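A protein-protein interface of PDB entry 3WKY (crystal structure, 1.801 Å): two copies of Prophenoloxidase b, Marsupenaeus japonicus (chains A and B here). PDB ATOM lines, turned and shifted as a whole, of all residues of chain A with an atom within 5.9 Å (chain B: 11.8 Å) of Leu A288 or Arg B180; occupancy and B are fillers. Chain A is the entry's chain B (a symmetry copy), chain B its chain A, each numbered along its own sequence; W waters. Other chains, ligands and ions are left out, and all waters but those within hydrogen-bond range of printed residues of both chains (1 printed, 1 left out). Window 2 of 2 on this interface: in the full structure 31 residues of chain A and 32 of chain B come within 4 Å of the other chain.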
ATOM      1  N   ARG A 284     -19.579   3.930   8.525  1.00  0.00           N
ATOM      2  CA  ARG A 284     -19.647   3.048   7.371  1.00  0.00           C
ATOM      3  C   ARG A 284     -20.968   3.314   6.661  1.00  0.00           C
ATOM      4  O   ARG A 284     -22.027   2.871   7.091  1.00  0.00           O
ATOM      5  CB  ARG A 284     -19.482   1.601   7.804  1.00  0.00           C
ATOM      6  CG  ARG A 284     -18.010   1.300   8.061  1.00  0.00           C
ATOM      7  CD  ARG A 284     -17.782   0.609   9.363  1.00  0.00           C
ATOM      8  NE  ARG A 284     -18.068   1.456  10.517  1.00  0.00           N
ATOM      9  CZ  ARG A 284     -18.135   0.974  11.752  1.00  0.00           C
ATOM     10  NH1 ARG A 284     -17.957  -0.325  11.949  1.00  0.00           N
ATOM     11  NH2 ARG A 284     -18.385   1.775  12.778  1.00  0.00           N
ATOM     12  N   GLU A 285     -20.886   4.111   5.599  1.00  0.00           N
ATOM     13  CA  GLU A 285     -22.064   4.580   4.895  1.00  0.00           C
ATOM     14  C   GLU A 285     -22.717   3.489   4.065  1.00  0.00           C
ATOM     15  O   GLU A 285     -22.176   2.388   3.902  1.00  0.00           O
ATOM     16  CB  GLU A 285     -21.686   5.731   3.954  1.00  0.00           C
ATOM     17  CG  GLU A 285     -21.903   7.115   4.533  1.00  0.00           C
ATOM     18  CD  GLU A 285     -23.379   7.481   4.670  1.00  0.00           C
ATOM     19  OE1 GLU A 285     -24.270   6.640   4.370  1.00  0.00           O
ATOM     20  OE2 GLU A 285     -23.650   8.619   5.090  1.00  0.00           O
ATOM     21  N   ILE A 286     -23.900   3.812   3.557  1.00  0.00           N
ATOM     22  CA  ILE A 286     -24.539   3.025   2.503  1.00  0.00           C
ATOM     23  C   ILE A 286     -24.703   3.969   1.318  1.00  0.00           C
ATOM     24  O   ILE A 286     -25.467   4.926   1.404  1.00  0.00           O
ATOM     25  CB  ILE A 286     -25.908   2.495   2.947  1.00  0.00           C
ATOM     26  CG1 ILE A 286     -25.741   1.552   4.143  1.00  0.00           C
ATOM     27  CG2 ILE A 286     -26.615   1.770   1.789  1.00  0.00           C
ATOM     28  CD1 ILE A 286     -27.027   1.308   4.907  1.00  0.00           C
ATOM     29  N   PRO A 287     -23.961   3.732   0.222  1.00  0.00           N
ATOM     30  CA  PRO A 287     -23.038   2.608   0.030  1.00  0.00           C
ATOM     31  C   PRO A 287     -21.723   2.769   0.795  1.00  0.00           C
ATOM     32  O   PRO A 287     -21.327   3.890   1.145  1.00  0.00           O
ATOM     33  CB  PRO A 287     -22.769   2.638  -1.474  1.00  0.00           C
ATOM     34  CG  PRO A 287     -22.853   4.095  -1.810  1.00  0.00           C
ATOM     35  CD  PRO A 287     -23.961   4.640  -0.940  1.00  0.00           C
ATOM     36  N   LEU A 288     -21.067   1.637   1.051  1.00  0.00           N
ATOM     37  CA  LEU A 288     -19.828   1.611   1.822  1.00  0.00           C
ATOM     38  C   LEU A 288     -18.731   2.487   1.217  1.00  0.00           C
ATOM     39  O   LEU A 288     -17.898   3.033   1.947  1.00  0.00           O
ATOM     40  CB  LEU A 288     -19.348   0.165   1.994  1.00  0.00           C
ATOM     41  CG  LEU A 288     -18.108  -0.118   2.842  1.00  0.00           C
ATOM     42  CD1 LEU A 288     -18.333   0.322   4.288  1.00  0.00           C
ATOM     43  CD2 LEU A 288     -17.783  -1.611   2.785  1.00  0.00           C
ATOM     44  N   VAL A 289     -18.731   2.663  -0.104  1.00  0.00           N
ATOM     45  CA  VAL A 289     -17.679   3.473  -0.719  1.00  0.00           C
ATOM     46  C   VAL A 289     -17.772   4.946  -0.302  1.00  0.00           C
ATOM     47  O   VAL A 289     -16.822   5.701  -0.487  1.00  0.00           O
ATOM     48  CB  VAL A 289     -17.659   3.360  -2.273  1.00  0.00           C
ATOM     49  CG1 VAL A 289     -17.258   1.948  -2.712  1.00  0.00           C
ATOM     50  CG2 VAL A 289     -19.022   3.745  -2.854  1.00  0.00           C
ATOM     51  N   ASP A 290     -18.904   5.355   0.271  1.00  0.00           N
ATOM     52  CA  ASP A 290     -19.062   6.745   0.725  1.00  0.00           C
ATOM     53  C   ASP A 290     -18.686   6.974   2.195  1.00  0.00           C
ATOM     54  O   ASP A 290     -19.041   8.003   2.783  1.00  0.00           O
ATOM     55  CB  ASP A 290     -20.505   7.227   0.530  1.00  0.00           C
ATOM     56  CG  ASP A 290     -20.890   7.363  -0.935  1.00  0.00           C
ATOM     57  OD1 ASP A 290     -20.004   7.271  -1.809  1.00  0.00           O
ATOM     58  OD2 ASP A 290     -22.093   7.570  -1.202  1.00  0.00           O
ATOM     59  N   SER A 291     -17.969   6.025   2.782  1.00  0.00           N
ATOM     60  CA  SER A 291     -17.635   6.061   4.211  1.00  0.00           C
ATOM     61  C   SER A 291     -16.519   7.021   4.582  1.00  0.00           C
ATOM     62  O   SER A 291     -15.766   7.481   3.716  1.00  0.00           O
ATOM     63  CB  SER A 291     -17.243   4.656   4.660  1.00  0.00           C
ATOM     64  OG  SER A 291     -18.326   3.800   4.416  1.00  0.00           O
ATOM     65  N   TYR A 293     -13.589   7.779   8.134  1.00  0.00           N
ATOM     66  CA  TYR A 293     -12.988   7.013   9.240  1.00  0.00           C
ATOM     67  C   TYR A 293     -12.308   7.921  10.247  1.00  0.00           C
ATOM     68  O   TYR A 293     -11.791   8.980   9.879  1.00  0.00           O
ATOM     69  CB  TYR A 293     -11.989   6.007   8.662  1.00  0.00           C
ATOM     70  CG  TYR A 293     -12.657   5.083   7.668  1.00  0.00           C
ATOM     71  CD1 TYR A 293     -12.819   5.447   6.330  1.00  0.00           C
ATOM     72  CD2 TYR A 293     -13.169   3.862   8.080  1.00  0.00           C
ATOM     73  CE1 TYR A 293     -13.479   4.585   5.423  1.00  0.00           C
ATOM     74  CE2 TYR A 293     -13.818   3.007   7.192  1.00  0.00           C
ATOM     75  CZ  TYR A 293     -13.964   3.371   5.870  1.00  0.00           C
ATOM     76  OH  TYR A 293     -14.620   2.496   5.010  1.00  0.00           O
ATOM     77  N   ALA A 371     -22.575   2.229  11.774  1.00  0.00           N
ATOM     78  CA  ALA A 371     -22.433   1.309  10.646  1.00  0.00           C
ATOM     79  C   ALA A 371     -23.770   1.089   9.954  1.00  0.00           C
ATOM     80  O   ALA A 371     -23.897   0.210   9.081  1.00  0.00           O
ATOM     81  CB  ALA A 371     -21.845  -0.007  11.094  1.00  0.00           C
ATOM     82  N   LYS A 372     -24.761   1.888  10.350  1.00  0.00           N
ATOM     83  CA  LYS A 372     -26.071   1.898   9.702  1.00  0.00           C
ATOM     84  C   LYS A 372     -26.699   0.507   9.654  1.00  0.00           C
ATOM     85  O   LYS A 372     -27.142   0.045   8.606  1.00  0.00           O
ATOM     86  CB  LYS A 372     -25.954   2.517   8.306  1.00  0.00           C
ATOM     87  CG  LYS A 372     -25.425   3.959   8.387  1.00  0.00           C
ATOM     88  CD  LYS A 372     -25.570   4.692   7.080  1.00  0.00           C
ATOM     89  CE  LYS A 372     -25.317   6.176   7.288  1.00  0.00           C
ATOM     90  NZ  LYS A 372     -26.283   6.748   8.260  1.00  0.00           N
ATOM     91  N   LYS A 373     -26.733  -0.137  10.816  1.00  0.00           N
ATOM     92  CA  LYS A 373     -27.265  -1.481  10.968  1.00  0.00           C
ATOM     93  C   LYS A 373     -28.743  -1.440  11.318  1.00  0.00           C
ATOM     94  O   LYS A 373     -29.466  -2.412  11.103  1.00  0.00           O
ATOM     95  CB  LYS A 373     -26.509  -2.195  12.099  1.00  0.00           C
ATOM     96  CG  LYS A 373     -25.042  -2.459  11.785  1.00  0.00           C
ATOM     97  CD  LYS A 373     -24.219  -2.825  13.035  1.00  0.00           C
ATOM     98  CE  LYS A 373     -24.860  -3.907  13.851  1.00  0.00           C
ATOM     99  NZ  LYS A 373     -23.965  -4.319  14.981  1.00  0.00           N
ATOM    100  N   SER B 172     -39.745  -6.613   6.281  1.00  0.00           N
ATOM    101  CA  SER B 172     -38.608  -6.627   7.210  1.00  0.00           C
ATOM    102  C   SER B 172     -37.445  -5.754   6.735  1.00  0.00           C
ATOM    103  O   SER B 172     -36.706  -5.205   7.553  1.00  0.00           O
ATOM    104  CB  SER B 172     -38.125  -8.061   7.460  1.00  0.00           C
ATOM    105  OG  SER B 172     -37.603  -8.633   6.273  1.00  0.00           O
ATOM    106  N   ASP B 173     -37.310  -5.607   5.416  1.00  0.00           N
ATOM    107  CA  ASP B 173     -36.313  -4.721   4.794  1.00  0.00           C
ATOM    108  C   ASP B 173     -36.388  -3.271   5.285  1.00  0.00           C
ATOM    109  O   ASP B 173     -35.689  -2.405   4.761  1.00  0.00           O
ATOM    110  CB  ASP B 173     -36.483  -4.701   3.263  1.00  0.00           C
ATOM    111  CG  ASP B 173     -35.811  -5.879   2.571  1.00  0.00           C
ATOM    112  OD1 ASP B 173     -34.796  -6.390   3.092  1.00  0.00           O
ATOM    113  OD2 ASP B 173     -36.293  -6.284   1.489  1.00  0.00           O
ATOM    114  N   GLU B 174     -37.228  -3.007   6.282  1.00  0.00           N
ATOM    115  CA  GLU B 174     -37.547  -1.636   6.663  1.00  0.00           C
ATOM    116  C   GLU B 174     -37.321  -1.291   8.143  1.00  0.00           C
ATOM    117  O   GLU B 174     -37.604  -0.166   8.553  1.00  0.00           O
ATOM    118  CB  GLU B 174     -38.993  -1.309   6.254  1.00  0.00           C
ATOM    119  CG  GLU B 174     -39.286  -1.537   4.767  1.00  0.00           C
ATOM    120  CD  GLU B 174     -40.770  -1.468   4.424  1.00  0.00           C
ATOM    121  OE1 GLU B 174     -41.330  -2.504   4.004  1.00  0.00           O
ATOM    122  OE2 GLU B 174     -41.372  -0.380   4.557  1.00  0.00           O
ATOM    123  N   THR B 175     -36.806  -2.227   8.939  1.00  0.00           N
ATOM    124  CA  THR B 175     -36.605  -1.981  10.384  1.00  0.00           C
ATOM    125  C   THR B 175     -35.181  -2.290  10.870  1.00  0.00           C
ATOM    126  O   THR B 175     -34.888  -2.253  12.071  1.00  0.00           O
ATOM    127  CB  THR B 175     -37.589  -2.797  11.233  1.00  0.00           C
ATOM    128  OG1 THR B 175     -37.472  -4.195  10.905  1.00  0.00           O
ATOM    129  CG2 THR B 175     -39.020  -2.330  10.977  1.00  0.00           C
ATOM    130  N   GLY B 176     -34.304  -2.595   9.925  1.00  0.00           N
ATOM    131  CA  GLY B 176     -32.943  -3.001  10.229  1.00  0.00           C
ATOM    132  C   GLY B 176     -32.401  -3.511   8.914  1.00  0.00           C
ATOM    133  O   GLY B 176     -33.170  -3.744   7.978  1.00  0.00           O
ATOM    134  N   LEU B 177     -31.089  -3.672   8.822  1.00  0.00           N
ATOM    135  CA  LEU B 177     -30.481  -4.082   7.564  1.00  0.00           C
ATOM    136  C   LEU B 177     -29.809  -5.434   7.751  1.00  0.00           C
ATOM    137  O   LEU B 177     -28.730  -5.510   8.340  1.00  0.00           O
ATOM    138  CB  LEU B 177     -29.455  -3.029   7.135  1.00  0.00           C
ATOM    139  CG  LEU B 177     -28.719  -3.247   5.815  1.00  0.00           C
ATOM    140  CD1 LEU B 177     -29.720  -3.434   4.690  1.00  0.00           C
ATOM    141  CD2 LEU B 177     -27.817  -2.058   5.540  1.00  0.00           C
ATOM    142  N   SER B 178     -30.432  -6.502   7.255  1.00  0.00           N
ATOM    143  CA  SER B 178     -29.906  -7.836   7.508  1.00  0.00           C
ATOM    144  C   SER B 178     -28.475  -7.993   7.011  1.00  0.00           C
ATOM    145  O   SER B 178     -27.676  -8.697   7.628  1.00  0.00           O
ATOM    146  CB  SER B 178     -30.805  -8.923   6.892  1.00  0.00           C
ATOM    147  OG  SER B 178     -31.990  -9.098   7.652  1.00  0.00           O
ATOM    148  N   SER B 179     -28.140  -7.336   5.903  1.00  0.00           N
ATOM    149  CA  SER B 179     -26.818  -7.553   5.326  1.00  0.00           C
ATOM    150  C   SER B 179     -25.700  -7.063   6.246  1.00  0.00           C
ATOM    151  O   SER B 179     -24.557  -7.496   6.101  1.00  0.00           O
ATOM    152  CB  SER B 179     -26.695  -6.921   3.936  1.00  0.00           C
ATOM    153  OG  SER B 179     -26.942  -5.531   3.984  1.00  0.00           O
ATOM    154  N   ARG B 180     -26.020  -6.171   7.188  1.00  0.00           N
ATOM    155  CA  ARG B 180     -25.008  -5.719   8.141  1.00  0.00           C
ATOM    156  C   ARG B 180     -25.281  -6.119   9.588  1.00  0.00           C
ATOM    157  O   ARG B 180     -24.501  -5.795  10.478  1.00  0.00           O
ATOM    158  CB  ARG B 180     -24.859  -4.200   8.087  1.00  0.00           C
ATOM    159  CG  ARG B 180     -24.525  -3.702   6.730  1.00  0.00           C
ATOM    160  CD  ARG B 180     -24.149  -2.245   6.791  1.00  0.00           C
ATOM    161  NE  ARG B 180     -23.542  -1.836   5.531  1.00  0.00           N
ATOM    162  CZ  ARG B 180     -23.047  -0.625   5.315  1.00  0.00           C
ATOM    163  NH1 ARG B 180     -23.088   0.283   6.287  1.00  0.00           N
ATOM    164  NH2 ARG B 180     -22.512  -0.331   4.136  1.00  0.00           N
ATOM    165  N   SER B 181     -26.384  -6.821   9.818  1.00  0.00           N
ATOM    166  CA  SER B 181     -26.823  -7.133  11.173  1.00  0.00           C
ATOM    167  C   SER B 181     -27.403  -8.544  11.214  1.00  0.00           C
ATOM    168  O   SER B 181     -28.589  -8.737  10.943  1.00  0.00           O
ATOM    169  CB  SER B 181     -27.877  -6.114  11.613  1.00  0.00           C
ATOM    170  OG  SER B 181     -28.379  -6.396  12.906  1.00  0.00           O
ATOM    171  N   PRO B 182     -26.568  -9.536  11.542  1.00  0.00           N
ATOM    172  CA  PRO B 182     -27.050 -10.925  11.568  1.00  0.00           C
ATOM    173  C   PRO B 182     -28.310 -11.093  12.432  1.00  0.00           C
ATOM    174  O   PRO B 182     -29.192 -11.867  12.055  1.00  0.00           O
ATOM    175  CB  PRO B 182     -25.874 -11.684  12.184  1.00  0.00           C
ATOM    176  CG  PRO B 182     -24.665 -10.916  11.727  1.00  0.00           C
ATOM    177  CD  PRO B 182     -25.104  -9.453  11.710  1.00  0.00           C
ATOM    178  N   GLU B 183     -28.413 -10.375  13.547  1.00  0.00           N
ATOM    179  CA  GLU B 183     -29.592 -10.542  14.410  1.00  0.00           C
ATOM    180  C   GLU B 183     -30.895 -10.152  13.726  1.00  0.00           C
ATOM    181  O   GLU B 183     -31.966 -10.623  14.109  1.00  0.00           O
ATOM    182  CB  GLU B 183     -29.441  -9.761  15.713  1.00  0.00           C
ATOM    183  CG  GLU B 183     -28.366 -10.321  16.619  1.00  0.00           C
ATOM    184  CD  GLU B 183     -28.670 -11.732  17.096  1.00  0.00           C
ATOM    185  OE1 GLU B 183     -29.861 -12.146  17.111  1.00  0.00           O
ATOM    186  OE2 GLU B 183     -27.704 -12.426  17.473  1.00  0.00           O
ATOM    187  N   HIS B 184     -30.810  -9.286  12.720  1.00  0.00           N
ATOM    188  CA  HIS B 184     -32.008  -8.886  11.988  1.00  0.00           C
ATOM    189  C   HIS B 184     -32.574 -10.028  11.135  1.00  0.00           C
ATOM    190  O   HIS B 184     -33.754  -9.989  10.781  1.00  0.00           O
ATOM    191  CB  HIS B 184     -31.756  -7.635  11.136  1.00  0.00           C
ATOM    192  CG  HIS B 184     -33.003  -7.039  10.567  1.00  0.00           C
ATOM    193  ND1 HIS B 184     -33.373  -7.211   9.250  1.00  0.00           N
ATOM    194  CD2 HIS B 184     -33.981  -6.296  11.141  1.00  0.00           C
ATOM    195  CE1 HIS B 184     -34.519  -6.586   9.033  1.00  0.00           C
ATOM    196  NE2 HIS B 184     -34.910  -6.025  10.163  1.00  0.00           N
ATOM    197  N   ARG B 185     -31.750 -11.036  10.828  1.00  0.00           N
ATOM    198  CA  ARG B 185     -32.197 -12.189  10.033  1.00  0.00           C
ATOM    199  C   ARG B 185     -33.344 -12.941  10.709  1.00  0.00           C
ATOM    200  O   ARG B 185     -34.115 -13.637  10.040  1.00  0.00           O
ATOM    201  CB  ARG B 185     -31.048 -13.178   9.712  1.00  0.00           C
ATOM    202  CG  ARG B 185     -29.959 -12.655   8.732  1.00  0.00           C
ATOM    203  CD  ARG B 185     -29.447 -13.751   7.746  1.00  0.00           C
ATOM    204  NE  ARG B 185     -28.737 -14.889   8.361  1.00  0.00           N
ATOM    205  CZ  ARG B 185     -27.472 -14.865   8.788  1.00  0.00           C
ATOM    206  NH1 ARG B 185     -26.730 -13.750   8.720  1.00  0.00           N
ATOM    207  NH2 ARG B 185     -26.940 -15.960   9.309  1.00  0.00           N
ATOM    208  N   VAL B 186     -33.459 -12.809  12.028  1.00  0.00           N
ATOM    209  CA  VAL B 186     -34.503 -13.529  12.761  1.00  0.00           C
ATOM    210  C   VAL B 186     -35.534 -12.556  13.360  1.00  0.00           C
ATOM    211  O   VAL B 186     -36.378 -12.925  14.180  1.00  0.00           O
ATOM    212  CB  VAL B 186     -33.882 -14.599  13.749  1.00  0.00           C
ATOM    213  CG1 VAL B 186     -32.991 -13.971  14.791  1.00  0.00           C
ATOM    214  CG2 VAL B 186     -34.932 -15.523  14.381  1.00  0.00           C
ATOM    215  N   SER B 187     -35.502 -11.309  12.897  1.00  0.00           N
ATOM    216  CA  SER B 187     -36.452 -10.316  13.382  1.00  0.00           C
ATOM    217  C   SER B 187     -37.901 -10.661  13.012  1.00  0.00           C
ATOM    218  O   SER B 187     -38.817 -10.333  13.758  1.00  0.00           O
ATOM    219  CB  SER B 187     -36.087  -8.898  12.916  1.00  0.00           C
ATOM    220  OG  SER B 187     -36.329  -8.721  11.534  1.00  0.00           O
ATOM    221  N   ARG B 190     -38.929 -12.858  16.055  1.00  0.00           N
ATOM    222  CA  ARG B 190     -39.004 -12.116  17.309  1.00  0.00           C
ATOM    223  C   ARG B 190     -40.131 -11.072  17.296  1.00  0.00           C
ATOM    224  O   ARG B 190     -40.760 -10.810  18.323  1.00  0.00           O
ATOM    225  CB  ARG B 190     -37.662 -11.412  17.612  1.00  0.00           C
ATOM    226  CG  ARG B 190     -36.496 -12.359  17.944  1.00  0.00           C
ATOM    227  CD  ARG B 190     -35.374 -11.564  18.656  1.00  0.00           C
ATOM    228  NE  ARG B 190     -35.012 -10.432  17.804  1.00  0.00           N
ATOM    229  CZ  ARG B 190     -33.991 -10.436  16.946  1.00  0.00           C
ATOM    230  NH1 ARG B 190     -33.158 -11.472  16.882  1.00  0.00           N
ATOM    231  NH2 ARG B 190     -33.777  -9.380  16.174  1.00  0.00           N
ATOM    232  N   LEU B 242     -27.370 -19.004  11.832  1.00  0.00           N
ATOM    233  CA  LEU B 242     -26.885 -18.215  12.967  1.00  0.00           C
ATOM    234  C   LEU B 242     -26.418 -19.147  14.078  1.00  0.00           C
ATOM    235  O   LEU B 242     -26.874 -20.286  14.177  1.00  0.00           O
ATOM    236  CB  LEU B 242     -27.988 -17.303  13.509  1.00  0.00           C
ATOM    237  CG  LEU B 242     -28.484 -16.195  12.595  1.00  0.00           C
ATOM    238  CD1 LEU B 242     -29.767 -15.588  13.167  1.00  0.00           C
ATOM    239  CD2 LEU B 242     -27.415 -15.129  12.434  1.00  0.00           C
ATOM    240  N   GLN B 256     -23.600  -6.522  23.494  1.00  0.00           N
ATOM    241  CA  GLN B 256     -23.066  -6.236  22.160  1.00  0.00           C
ATOM    242  C   GLN B 256     -24.140  -5.730  21.184  1.00  0.00           C
ATOM    243  O   GLN B 256     -23.959  -4.712  20.512  1.00  0.00           O
ATOM    244  CB  GLN B 256     -22.380  -7.488  21.596  1.00  0.00           C
ATOM    245  CG  GLN B 256     -21.976  -7.390  20.133  1.00  0.00           C
ATOM    246  CD  GLN B 256     -21.303  -8.671  19.637  1.00  0.00           C
ATOM    247  OE1 GLN B 256     -20.619  -9.359  20.393  1.00  0.00           O
ATOM    248  NE2 GLN B 256     -21.508  -8.994  18.369  1.00  0.00           N
ATOM    249  N   ASP B 257     -25.271  -6.426  21.113  1.00  0.00           N
ATOM    250  CA  ASP B 257     -26.286  -6.077  20.121  1.00  0.00           C
ATOM    251  C   ASP B 257     -27.395  -5.214  20.696  1.00  0.00           C
ATOM    252  O   ASP B 257     -28.149  -5.655  21.575  1.00  0.00           O
ATOM    253  CB  ASP B 257     -26.883  -7.342  19.505  1.00  0.00           C
ATOM    254  CG  ASP B 257     -25.835  -8.199  18.849  1.00  0.00           C
ATOM    255  OD1 ASP B 257     -25.030  -7.646  18.067  1.00  0.00           O
ATOM    256  OD2 ASP B 257     -25.796  -9.411  19.139  1.00  0.00           O
ATOM    257  N   GLY B 258     -27.488  -3.985  20.190  1.00  0.00           N
ATOM    258  CA  GLY B 258     -28.552  -3.092  20.594  1.00  0.00           C
ATOM    259  C   GLY B 258     -29.825  -3.447  19.839  1.00  0.00           C
ATOM    260  O   GLY B 258     -29.884  -4.465  19.131  1.00  0.00           O
ATOM    261  N   PHE B 260     -33.321  -1.194  18.017  1.00  0.00           N
ATOM    262  CA  PHE B 260     -34.114  -0.002  17.781  1.00  0.00           C
ATOM    263  C   PHE B 260     -35.503  -0.473  17.321  1.00  0.00           C
ATOM    264  O   PHE B 260     -35.676  -0.899  16.181  1.00  0.00           O
ATOM    265  CB  PHE B 260     -33.440   0.857  16.709  1.00  0.00           C
ATOM    266  CG  PHE B 260     -32.138   1.500  17.166  1.00  0.00           C
ATOM    267  CD1 PHE B 260     -30.990   0.733  17.387  1.00  0.00           C
ATOM    268  CD2 PHE B 260     -32.071   2.872  17.372  1.00  0.00           C
ATOM    269  CE1 PHE B 260     -29.797   1.342  17.818  1.00  0.00           C
ATOM    270  CE2 PHE B 260     -30.892   3.485  17.800  1.00  0.00           C
ATOM    271  CZ  PHE B 260     -29.758   2.730  18.020  1.00  0.00           C
ATOM    272  N   ASP B 276     -25.881  -0.386  20.215  1.00  0.00           N
ATOM    273  CA  ASP B 276     -24.903  -1.465  20.366  1.00  0.00           C
ATOM    274  C   ASP B 276     -23.911  -1.128  21.489  1.00  0.00           C
ATOM    275  O   ASP B 276     -23.589   0.052  21.725  1.00  0.00           O
ATOM    276  CB  ASP B 276     -24.109  -1.681  19.073  1.00  0.00           C
ATOM    277  CG  ASP B 276     -24.930  -2.300  17.947  1.00  0.00           C
ATOM    278  OD1 ASP B 276     -25.954  -2.981  18.184  1.00  0.00           O
ATOM    279  OD2 ASP B 276     -24.514  -2.131  16.785  1.00  0.00           O
ATOM    280  N   PRO B 391     -33.519  -8.692  20.559  1.00  0.00           N
ATOM    281  CA  PRO B 391     -32.625  -9.860  20.651  1.00  0.00           C
ATOM    282  C   PRO B 391     -32.124 -10.126  22.073  1.00  0.00           C
ATOM    283  O   PRO B 391     -31.866 -11.281  22.429  1.00  0.00           O
ATOM    284  CB  PRO B 391     -31.459  -9.504  19.708  1.00  0.00           C
ATOM    285  CG  PRO B 391     -31.556  -7.966  19.530  1.00  0.00           C
ATOM    286  CD  PRO B 391     -33.049  -7.711  19.560  1.00  0.00           C
HETATM  287  O   HOH W   1     -30.552  -4.635  12.898  1.00  0.00           O
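Among the printed residues, pairs that only touch across the chains: Ile A286 with Leu B177 (3.5 Å), Ile A286 with Arg B180 (3.6 Å), Leu A288 with Arg B180 (3.9 Å), Lys A372 with Leu B177 (3.8 Å), Lys A373 with Gly B176 (3.6 Å) and Lys A373 with Arg B180 (3.6 Å).
The backbone carbonyl oxygen (O) of Ala A371 is in hydrogen-bond range of the guanidinium group (NH1) of Arg B180 (2.9 Å). NH1 of Arg B180 is in hydrogen-bond range of O of Arg A284. O of Glu A285 sits at hydrogen-bond distance from NH2 of Arg B180. The backbone NH (N) of Leu B177 sits at hydrogen-bond distance from the backbone carbonyl oxygen (O) of Lys A373, at 3.1 Å. The side-chain carboxylate (OD2) of Asp B276 lies within salt-bridge range of the side-chain amino group (NZ) of Lys A373, 2.9 Å away.
Printed residues of chain B within 4 Å of Glu A285: Arg B180. Of chain B, only Leu B177 and Arg B180 come within 4 Å of Ile A286. No residue of chain B comes within 4 Å of Pro A287. Of the printed residues of chain B, Leu A288 touches Arg B180 (3.9 Å). No residue of chain B comes within 4 Å of Val A289. Ala A371 touches just one residue of chain B: Arg B180. Of chain B, only Leu B177 comes within 4 Å of Lys A372. Of chain B, only Gly B176, Leu B177, Arg B180 and Asp B276 come within 4 Å of Lys A373. Printed residues of chain A within 4 Å of Gly B176: Lys A373 (3.6 Å). Of chain A, only Arg A284, Glu A285, Ile A286, Leu A288, Ala A371 and Lys A373 come within 4 Å of Arg B180. Printed residues of chain A within 4 Å of Asp B276: Lys A373. The nearest printed residue of chain B that does not touch Glu A285 is Leu B177 (7.4 Å).
Water W1 lies within hydrogen-bond range of OG of Ser B181 (2.8 Å) and O of Lys A373 (3.1 Å).
Of the 24 printed residues of chain B, 4 touch a printed residue of chain A. Hydrophobic or aromatic side chains of chain B that line the printed part of chain A: Leu B177. Of the 12 printed residues of chain A, 7 touch a printed residue of chain B. Hydrophobic or aromatic side chains of chain A within 4 Å of the printed part of chain B: Ile A286 and Leu A288. Among the printed residues, Asp or Glu carboxylates within 4 Å of a Lys or Arg side-chain nitrogen of the other chain: Lys A373 with Asp B276.
No position is printed for both chains.
The backbone NH (N) of Gly B176 is in hydrogen-bond range of a ring nitrogen (NE2) of His B184 (3.5 Å). The side-chain hydroxyl (OG) of Ser A291 lies within hydrogen-bond range of the backbone NH (N) of Glu A285 (2.8 Å). The backbone NH (N) of Gly B258 is in hydrogen-bond range of the side-chain carboxylate (OD1) of Asp B276. O of Leu A288 lies within hydrogen-bond range of OG of Ser A291 (2.6 Å).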
